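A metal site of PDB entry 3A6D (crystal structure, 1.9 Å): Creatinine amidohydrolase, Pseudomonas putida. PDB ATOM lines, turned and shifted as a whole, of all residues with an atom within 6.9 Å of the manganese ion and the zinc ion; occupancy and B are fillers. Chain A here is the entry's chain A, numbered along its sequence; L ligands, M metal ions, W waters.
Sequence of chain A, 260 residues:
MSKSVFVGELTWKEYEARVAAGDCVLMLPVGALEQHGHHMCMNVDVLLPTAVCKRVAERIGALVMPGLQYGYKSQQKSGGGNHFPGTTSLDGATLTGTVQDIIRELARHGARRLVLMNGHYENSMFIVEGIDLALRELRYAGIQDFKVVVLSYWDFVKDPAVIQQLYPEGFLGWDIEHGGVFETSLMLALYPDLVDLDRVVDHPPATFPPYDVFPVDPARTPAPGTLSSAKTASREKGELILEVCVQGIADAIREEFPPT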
ATOM      1  N   GLY A  31       3.855   4.018 -19.754  1.00  0.00           N
ATOM      2  CA  GLY A  31       4.356   3.241 -18.644  1.00  0.00           C
ATOM      3  C   GLY A  31       4.996   3.991 -17.494  1.00  0.00           C
ATOM      4  O   GLY A  31       4.479   5.007 -17.025  1.00  0.00           O
ATOM      5  N   ALA A  32       6.133   3.458 -17.030  1.00  0.00           N
ATOM      6  CA  ALA A  32       6.877   4.024 -15.915  1.00  0.00           C
ATOM      7  C   ALA A  32       8.141   3.231 -15.648  1.00  0.00           C
ATOM      8  O   ALA A  32       8.293   2.115 -16.147  1.00  0.00           O
ATOM      9  CB  ALA A  32       6.013   4.038 -14.649  1.00  0.00           C
ATOM     10  N   GLU A  34       9.769   1.852 -12.475  1.00  0.00           N
ATOM     11  CA  GLU A  34       9.391   1.671 -11.078  1.00  0.00           C
ATOM     12  C   GLU A  34       9.846   0.332 -10.505  1.00  0.00           C
ATOM     13  O   GLU A  34       9.861  -0.683 -11.203  1.00  0.00           O
ATOM     14  CB  GLU A  34       7.858   1.776 -11.006  1.00  0.00           C
ATOM     15  CG  GLU A  34       7.209   1.680  -9.635  1.00  0.00           C
ATOM     16  CD  GLU A  34       5.703   1.497  -9.763  1.00  0.00           C
ATOM     17  OE1 GLU A  34       4.951   1.984  -8.900  1.00  0.00           O
ATOM     18  OE2 GLU A  34       5.278   0.855 -10.746  1.00  0.00           O
ATOM     19  N   GLN A  35      10.195   0.324  -9.219  1.00  0.00           N
ATOM     20  CA  GLN A  35      10.627  -0.900  -8.563  1.00  0.00           C
ATOM     21  C   GLN A  35       9.521  -1.945  -8.694  1.00  0.00           C
ATOM     22  O   GLN A  35       8.337  -1.614  -8.639  1.00  0.00           O
ATOM     23  CB  GLN A  35      10.937  -0.630  -7.088  1.00  0.00           C
ATOM     24  CG  GLN A  35       9.743  -0.214  -6.214  1.00  0.00           C
ATOM     25  CD  GLN A  35       8.884  -1.388  -5.765  1.00  0.00           C
ATOM     26  OE1 GLN A  35       9.360  -2.523  -5.685  1.00  0.00           O
ATOM     27  NE2 GLN A  35       7.620  -1.120  -5.443  1.00  0.00           N
ATOM     28  N   HIS A  36       9.926  -3.197  -8.878  1.00  0.00           N
ATOM     29  CA  HIS A  36       8.979  -4.311  -8.991  1.00  0.00           C
ATOM     30  C   HIS A  36       9.454  -5.519  -8.195  1.00  0.00           C
ATOM     31  O   HIS A  36       9.451  -6.636  -8.712  1.00  0.00           O
ATOM     32  CB  HIS A  36       8.782  -4.715 -10.449  1.00  0.00           C
ATOM     33  CG  HIS A  36       7.771  -3.885 -11.177  1.00  0.00           C
ATOM     34  ND1 HIS A  36       8.033  -2.593 -11.582  1.00  0.00           N
ATOM     35  CD2 HIS A  36       6.498  -4.138 -11.531  1.00  0.00           C
ATOM     36  CE1 HIS A  36       6.956  -2.083 -12.157  1.00  0.00           C
ATOM     37  NE2 HIS A  36       6.011  -3.010 -12.138  1.00  0.00           N
ATOM     38  N   MET A  40      11.911  -8.983 -10.287  1.00  0.00           N
ATOM     39  CA  MET A  40      11.694  -8.428 -11.624  1.00  0.00           C
ATOM     40  C   MET A  40      12.395  -7.099 -11.846  1.00  0.00           C
ATOM     41  O   MET A  40      12.733  -6.410 -10.890  1.00  0.00           O
ATOM     42  CB  MET A  40      10.198  -8.212 -11.892  1.00  0.00           C
ATOM     43  CG  MET A  40       9.387  -9.452 -12.135  1.00  0.00           C
ATOM     44  SD  MET A  40       7.909  -9.033 -13.056  1.00  0.00           S
ATOM     45  CE  MET A  40       6.946  -8.189 -11.801  1.00  0.00           C
ATOM     46  N   VAL A  44       8.966  -2.885 -16.415  1.00  0.00           N
ATOM     47  CA  VAL A  44       7.770  -3.706 -16.640  1.00  0.00           C
ATOM     48  C   VAL A  44       6.589  -2.931 -17.212  1.00  0.00           C
ATOM     49  O   VAL A  44       5.965  -3.347 -18.193  1.00  0.00           O
ATOM     50  CB  VAL A  44       7.325  -4.383 -15.315  1.00  0.00           C
ATOM     51  CG1 VAL A  44       5.984  -5.063 -15.498  1.00  0.00           C
ATOM     52  CG2 VAL A  44       8.379  -5.398 -14.869  1.00  0.00           C
ATOM     53  N   ASP A  45       6.270  -1.790 -16.606  1.00  0.00           N
ATOM     54  CA  ASP A  45       5.120  -0.991 -17.047  1.00  0.00           C
ATOM     55  C   ASP A  45       5.214  -0.435 -18.450  1.00  0.00           C
ATOM     56  O   ASP A  45       4.208   0.022 -18.994  1.00  0.00           O
ATOM     57  CB  ASP A  45       4.845   0.126 -16.038  1.00  0.00           C
ATOM     58  CG  ASP A  45       4.357  -0.420 -14.719  1.00  0.00           C
ATOM     59  OD1 ASP A  45       4.205  -1.657 -14.639  1.00  0.00           O
ATOM     60  OD2 ASP A  45       4.122   0.358 -13.788  1.00  0.00           O
ATOM     61  N   LEU A  48       5.215  -4.344 -20.898  1.00  0.00           N
ATOM     62  CA  LEU A  48       3.941  -5.031 -21.046  1.00  0.00           C
ATOM     63  C   LEU A  48       2.917  -4.334 -21.954  1.00  0.00           C
ATOM     64  O   LEU A  48       2.412  -4.961 -22.880  1.00  0.00           O
ATOM     65  CB  LEU A  48       3.346  -5.323 -19.662  1.00  0.00           C
ATOM     66  CG  LEU A  48       4.275  -6.199 -18.796  1.00  0.00           C
ATOM     67  CD1 LEU A  48       3.568  -6.603 -17.505  1.00  0.00           C
ATOM     68  CD2 LEU A  48       4.687  -7.448 -19.566  1.00  0.00           C
ATOM     69  N   SER A  74       4.769   6.798  -7.887  1.00  0.00           N
ATOM     70  CA  SER A  74       4.246   5.553  -7.358  1.00  0.00           C
ATOM     71  C   SER A  74       3.521   5.843  -6.042  1.00  0.00           C
ATOM     72  O   SER A  74       4.025   6.591  -5.208  1.00  0.00           O
ATOM     73  CB  SER A  74       5.411   4.576  -7.108  1.00  0.00           C
ATOM     74  OG  SER A  74       4.950   3.329  -6.611  1.00  0.00           O
ATOM     75  N   SER A  78      -0.856   1.266  -4.330  1.00  0.00           N
ATOM     76  CA  SER A  78      -0.947   0.666  -5.649  1.00  0.00           C
ATOM     77  C   SER A  78       0.391   0.300  -6.285  1.00  0.00           C
ATOM     78  O   SER A  78       0.438  -0.506  -7.211  1.00  0.00           O
ATOM     79  CB  SER A  78      -1.725   1.589  -6.595  1.00  0.00           C
ATOM     80  OG  SER A  78      -1.207   2.913  -6.570  1.00  0.00           O
ATOM     81  N   GLY A  79       1.472   0.895  -5.795  1.00  0.00           N
ATOM     82  CA  GLY A  79       2.782   0.612  -6.367  1.00  0.00           C
ATOM     83  C   GLY A  79       3.927   0.555  -5.375  1.00  0.00           C
ATOM     84  O   GLY A  79       5.088   0.561  -5.783  1.00  0.00           O
ATOM     85  N   GLY A 119      -0.053   1.359 -18.590  1.00  0.00           N
ATOM     86  CA  GLY A 119       0.495   0.165 -17.981  1.00  0.00           C
ATOM     87  C   GLY A 119       0.925   0.421 -16.540  1.00  0.00           C
ATOM     88  O   GLY A 119       1.379  -0.493 -15.851  1.00  0.00           O
ATOM     89  N   HIS A 120       0.772   1.670 -16.093  1.00  0.00           N
ATOM     90  CA  HIS A 120       1.149   2.082 -14.734  1.00  0.00           C
ATOM     91  C   HIS A 120      -0.092   2.668 -14.056  1.00  0.00           C
ATOM     92  O   HIS A 120      -0.564   3.746 -14.409  1.00  0.00           O
ATOM     93  CB  HIS A 120       2.281   3.128 -14.812  1.00  0.00           C
ATOM     94  CG  HIS A 120       2.705   3.685 -13.483  1.00  0.00           C
ATOM     95  ND1 HIS A 120       3.169   2.893 -12.452  1.00  0.00           N
ATOM     96  CD2 HIS A 120       2.799   4.966 -13.040  1.00  0.00           C
ATOM     97  CE1 HIS A 120       3.528   3.658 -11.430  1.00  0.00           C
ATOM     98  NE2 HIS A 120       3.312   4.916 -11.764  1.00  0.00           N
ATOM     99  N   TYR A 121      -0.613   1.920 -13.091  1.00  0.00           N
ATOM    100  CA  TYR A 121      -1.830   2.274 -12.357  1.00  0.00           C
ATOM    101  C   TYR A 121      -2.021   3.766 -12.059  1.00  0.00           C
ATOM    102  O   TYR A 121      -3.076   4.326 -12.350  1.00  0.00           O
ATOM    103  CB  TYR A 121      -1.849   1.491 -11.039  1.00  0.00           C
ATOM    104  CG  TYR A 121      -3.191   1.483 -10.338  1.00  0.00           C
ATOM    105  CD1 TYR A 121      -4.073   0.415 -10.492  1.00  0.00           C
ATOM    106  CD2 TYR A 121      -3.564   2.532  -9.504  1.00  0.00           C
ATOM    107  CE1 TYR A 121      -5.298   0.386  -9.817  1.00  0.00           C
ATOM    108  CE2 TYR A 121      -4.788   2.520  -8.826  1.00  0.00           C
ATOM    109  CZ  TYR A 121      -5.646   1.444  -8.998  1.00  0.00           C
ATOM    110  OH  TYR A 121      -6.849   1.426  -8.322  1.00  0.00           O
ATOM    111  N   GLU A 122      -0.991   4.399 -11.512  1.00  0.00           N
ATOM    112  CA  GLU A 122      -1.040   5.804 -11.130  1.00  0.00           C
ATOM    113  C   GLU A 122      -1.135   6.863 -12.246  1.00  0.00           C
ATOM    114  O   GLU A 122      -1.475   8.013 -11.952  1.00  0.00           O
ATOM    115  CB  GLU A 122       0.159   6.138 -10.233  1.00  0.00           C
ATOM    116  CG  GLU A 122       0.144   5.424  -8.873  1.00  0.00           C
ATOM    117  CD  GLU A 122       0.770   4.037  -8.905  1.00  0.00           C
ATOM    118  OE1 GLU A 122       0.788   3.392  -9.975  1.00  0.00           O
ATOM    119  OE2 GLU A 122       1.228   3.574  -7.844  1.00  0.00           O
ATOM    120  N   TYR A 153      -4.682  -1.964 -19.628  1.00  0.00           N
ATOM    121  CA  TYR A 153      -4.856  -3.309 -20.167  1.00  0.00           C
ATOM    122  C   TYR A 153      -5.377  -4.417 -19.252  1.00  0.00           C
ATOM    123  O   TYR A 153      -6.131  -5.276 -19.701  1.00  0.00           O
ATOM    124  CB  TYR A 153      -3.565  -3.735 -20.889  1.00  0.00           C
ATOM    125  CG  TYR A 153      -2.425  -4.127 -19.993  1.00  0.00           C
ATOM    126  CD1 TYR A 153      -2.226  -5.456 -19.619  1.00  0.00           C
ATOM    127  CD2 TYR A 153      -1.537  -3.166 -19.500  1.00  0.00           C
ATOM    128  CE1 TYR A 153      -1.192  -5.825 -18.778  1.00  0.00           C
ATOM    129  CE2 TYR A 153      -0.481  -3.524 -18.658  1.00  0.00           C
ATOM    130  CZ  TYR A 153      -0.323  -4.861 -18.301  1.00  0.00           C
ATOM    131  OH  TYR A 153       0.689  -5.231 -17.451  1.00  0.00           O
ATOM    132  N   TRP A 154      -5.012  -4.402 -17.968  1.00  0.00           N
ATOM    133  CA  TRP A 154      -5.485  -5.449 -17.069  1.00  0.00           C
ATOM    134  C   TRP A 154      -7.000  -5.456 -16.862  1.00  0.00           C
ATOM    135  O   TRP A 154      -7.571  -6.477 -16.473  1.00  0.00           O
ATOM    136  CB  TRP A 154      -4.777  -5.358 -15.711  1.00  0.00           C
ATOM    137  CG  TRP A 154      -4.877  -4.010 -15.066  1.00  0.00           C
ATOM    138  CD1 TRP A 154      -5.945  -3.505 -14.378  1.00  0.00           C
ATOM    139  CD2 TRP A 154      -3.868  -2.996 -15.056  1.00  0.00           C
ATOM    140  NE1 TRP A 154      -5.656  -2.219 -13.948  1.00  0.00           N
ATOM    141  CE2 TRP A 154      -4.397  -1.886 -14.351  1.00  0.00           C
ATOM    142  CE3 TRP A 154      -2.570  -2.911 -15.588  1.00  0.00           C
ATOM    143  CZ2 TRP A 154      -3.667  -0.706 -14.157  1.00  0.00           C
ATOM    144  CZ3 TRP A 154      -1.841  -1.731 -15.394  1.00  0.00           C
ATOM    145  CH2 TRP A 154      -2.401  -0.651 -14.682  1.00  0.00           C
ATOM    146  N   GLU A 177      -2.027  -5.612  -7.194  1.00  0.00           N
ATOM    147  CA  GLU A 177      -1.426  -6.429  -8.235  1.00  0.00           C
ATOM    148  C   GLU A 177      -0.164  -5.726  -8.779  1.00  0.00           C
ATOM    149  O   GLU A 177      -0.016  -5.540  -9.986  1.00  0.00           O
ATOM    150  CB  GLU A 177      -2.451  -6.665  -9.343  1.00  0.00           C
ATOM    151  CG  GLU A 177      -2.191  -7.896 -10.197  1.00  0.00           C
ATOM    152  CD  GLU A 177      -1.829  -9.120  -9.367  1.00  0.00           C
ATOM    153  OE1 GLU A 177      -2.690  -9.651  -8.640  1.00  0.00           O
ATOM    154  OE2 GLU A 177      -0.653  -9.541  -9.444  1.00  0.00           O
ATOM    155  N   HIS A 178       0.713  -5.330  -7.870  1.00  0.00           N
ATOM    156  CA  HIS A 178       1.970  -4.689  -8.261  1.00  0.00           C
ATOM    157  C   HIS A 178       3.104  -5.668  -7.993  1.00  0.00           C
ATOM    158  O   HIS A 178       3.411  -5.964  -6.835  1.00  0.00           O
ATOM    159  CB  HIS A 178       2.216  -3.407  -7.470  1.00  0.00           C
ATOM    160  CG  HIS A 178       3.555  -2.786  -7.751  1.00  0.00           C
ATOM    161  ND1 HIS A 178       3.878  -2.242  -8.977  1.00  0.00           N
ATOM    162  CD2 HIS A 178       4.671  -2.687  -6.980  1.00  0.00           C
ATOM    163  CE1 HIS A 178       5.138  -1.826  -8.949  1.00  0.00           C
ATOM    164  NE2 HIS A 178       5.634  -2.091  -7.751  1.00  0.00           N
ATOM    165  N   GLY A 179       3.717  -6.164  -9.065  1.00  0.00           N
ATOM    166  CA  GLY A 179       4.810  -7.107  -8.897  1.00  0.00           C
ATOM    167  C   GLY A 179       4.311  -8.457  -8.411  1.00  0.00           C
ATOM    168  O   GLY A 179       5.075  -9.247  -7.881  1.00  0.00           O
ATOM    169  N   GLU A 183       1.437  -9.367 -13.356  1.00  0.00           N
ATOM    170  CA  GLU A 183       2.574  -8.853 -14.116  1.00  0.00           C
ATOM    171  C   GLU A 183       3.697  -9.862 -14.241  1.00  0.00           C
ATOM    172  O   GLU A 183       4.288 -10.012 -15.311  1.00  0.00           O
ATOM    173  CB  GLU A 183       3.129  -7.574 -13.468  1.00  0.00           C
ATOM    174  CG  GLU A 183       2.170  -6.410 -13.471  1.00  0.00           C
ATOM    175  CD  GLU A 183       2.812  -5.155 -12.930  1.00  0.00           C
ATOM    176  OE1 GLU A 183       2.843  -4.151 -13.674  1.00  0.00           O
ATOM    177  OE2 GLU A 183       3.289  -5.172 -11.771  1.00  0.00           O
HETATM  178  C1  LIG L   1      -2.062  -3.088 -11.619  1.00  0.00           C
HETATM  179  N1  LIG L   1      -0.970  -2.369 -11.302  1.00  0.00           N
HETATM  180  C2  LIG L   1      -0.684  -1.955 -10.046  1.00  0.00           C
HETATM  181  N2  LIG L   1      -1.469  -2.214  -8.999  1.00  0.00           N
HETATM  182  N3  LIG L   1       0.427  -1.249  -9.855  1.00  0.00           N
HETATM  183 MN    MN M   1       3.441   0.662 -11.786  1.00  0.00          MN
HETATM  184 ZN    ZN M   2       3.974  -2.630 -12.751  1.00  0.00          ZN
HETATM  185  O   HOH W   1       2.929  -1.462 -11.298  1.00  0.00           O
HETATM  186  O   HOH W   2       0.922  -0.875 -12.861  1.00  0.00           O
HETATM  187  O   HOH W   3       2.401   1.050  -9.800  1.00  0.00           O
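ND1 of His 36 lies within hydrogen-bond range of O of Glu 34. NE2 of His 120 lies close to OE1 of Glu 122 (3.4 Å). N of Gly 179 sits at hydrogen-bond distance from OE2 of Glu 183 (2.9 Å). NE2 of His 178 sits at hydrogen-bond distance from O of Gln 35 (2.9 Å). The backbone carbonyl oxygen of Gly 79 is in hydrogen-bond range of a ring nitrogen (NE2) of His 178 (3.3 Å). OE1 of Glu 34 lies within hydrogen-bond range of OG of Ser 74, 2.7 Å away.
ND1 of His 178 touches the zinc ion, at 3.8 Å. Within 4 Å of the zinc ion: His 36, Asp 45, His 178 and Glu 183. The nearest printed residue that does not touch the zinc ion is Val 44 (4.2 Å).
Water W3 lies within hydrogen-bond range of OE1 of Glu 122 (2.8 Å), OE1 of Glu 34 (2.9 Å) and N3 of the ligand (3.0 Å). Water W1 bridges ND1 of His 178 (2.6 Å) and N3 of the ligand (2.9 Å). Water W2 lies within hydrogen-bond range of a nitrogen (N1) of the ligand (2.9 Å), the backbone carbonyl oxygen (O) of Gly 119 (3.0 Å) and the backbone NH (N) of Tyr 121 (3.2 Å).
The zinc ion is bound by the side-chain carboxylate (OE1) of Glu 183 (2.1 Å), the side-chain carboxylate (OD1) of Asp 45 (2.1 Å), water W1 (2.1 Å) and a ring nitrogen (NE2) of His 36 (2.2 Å). Slightly farther from the zinc ion lies the side-chain carboxylate (OE2) of Glu 183 (2.8 Å).
O of Ser 78 sits at hydrogen-bond distance from N3 of the ligand (2.7 Å).
Within 4 Å of the manganese ion: Glu 34, Asp 45 and His 120. The nearest printed residue that does not touch the manganese ion is His 178 (4.1 Å).
OE2 of Glu 34 binds the manganese ion, at 2.1 Å. The manganese ion is bound by OD2 of Asp 45, at 2.1 Å. Water W1 is bound to the manganese ion, at 2.2 Å. Water W3 is bound to the manganese ion. ND1 of His 120 is bound to the manganese ion, 2.3 Å away. The manganese ion has five donor atoms within binding distance.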
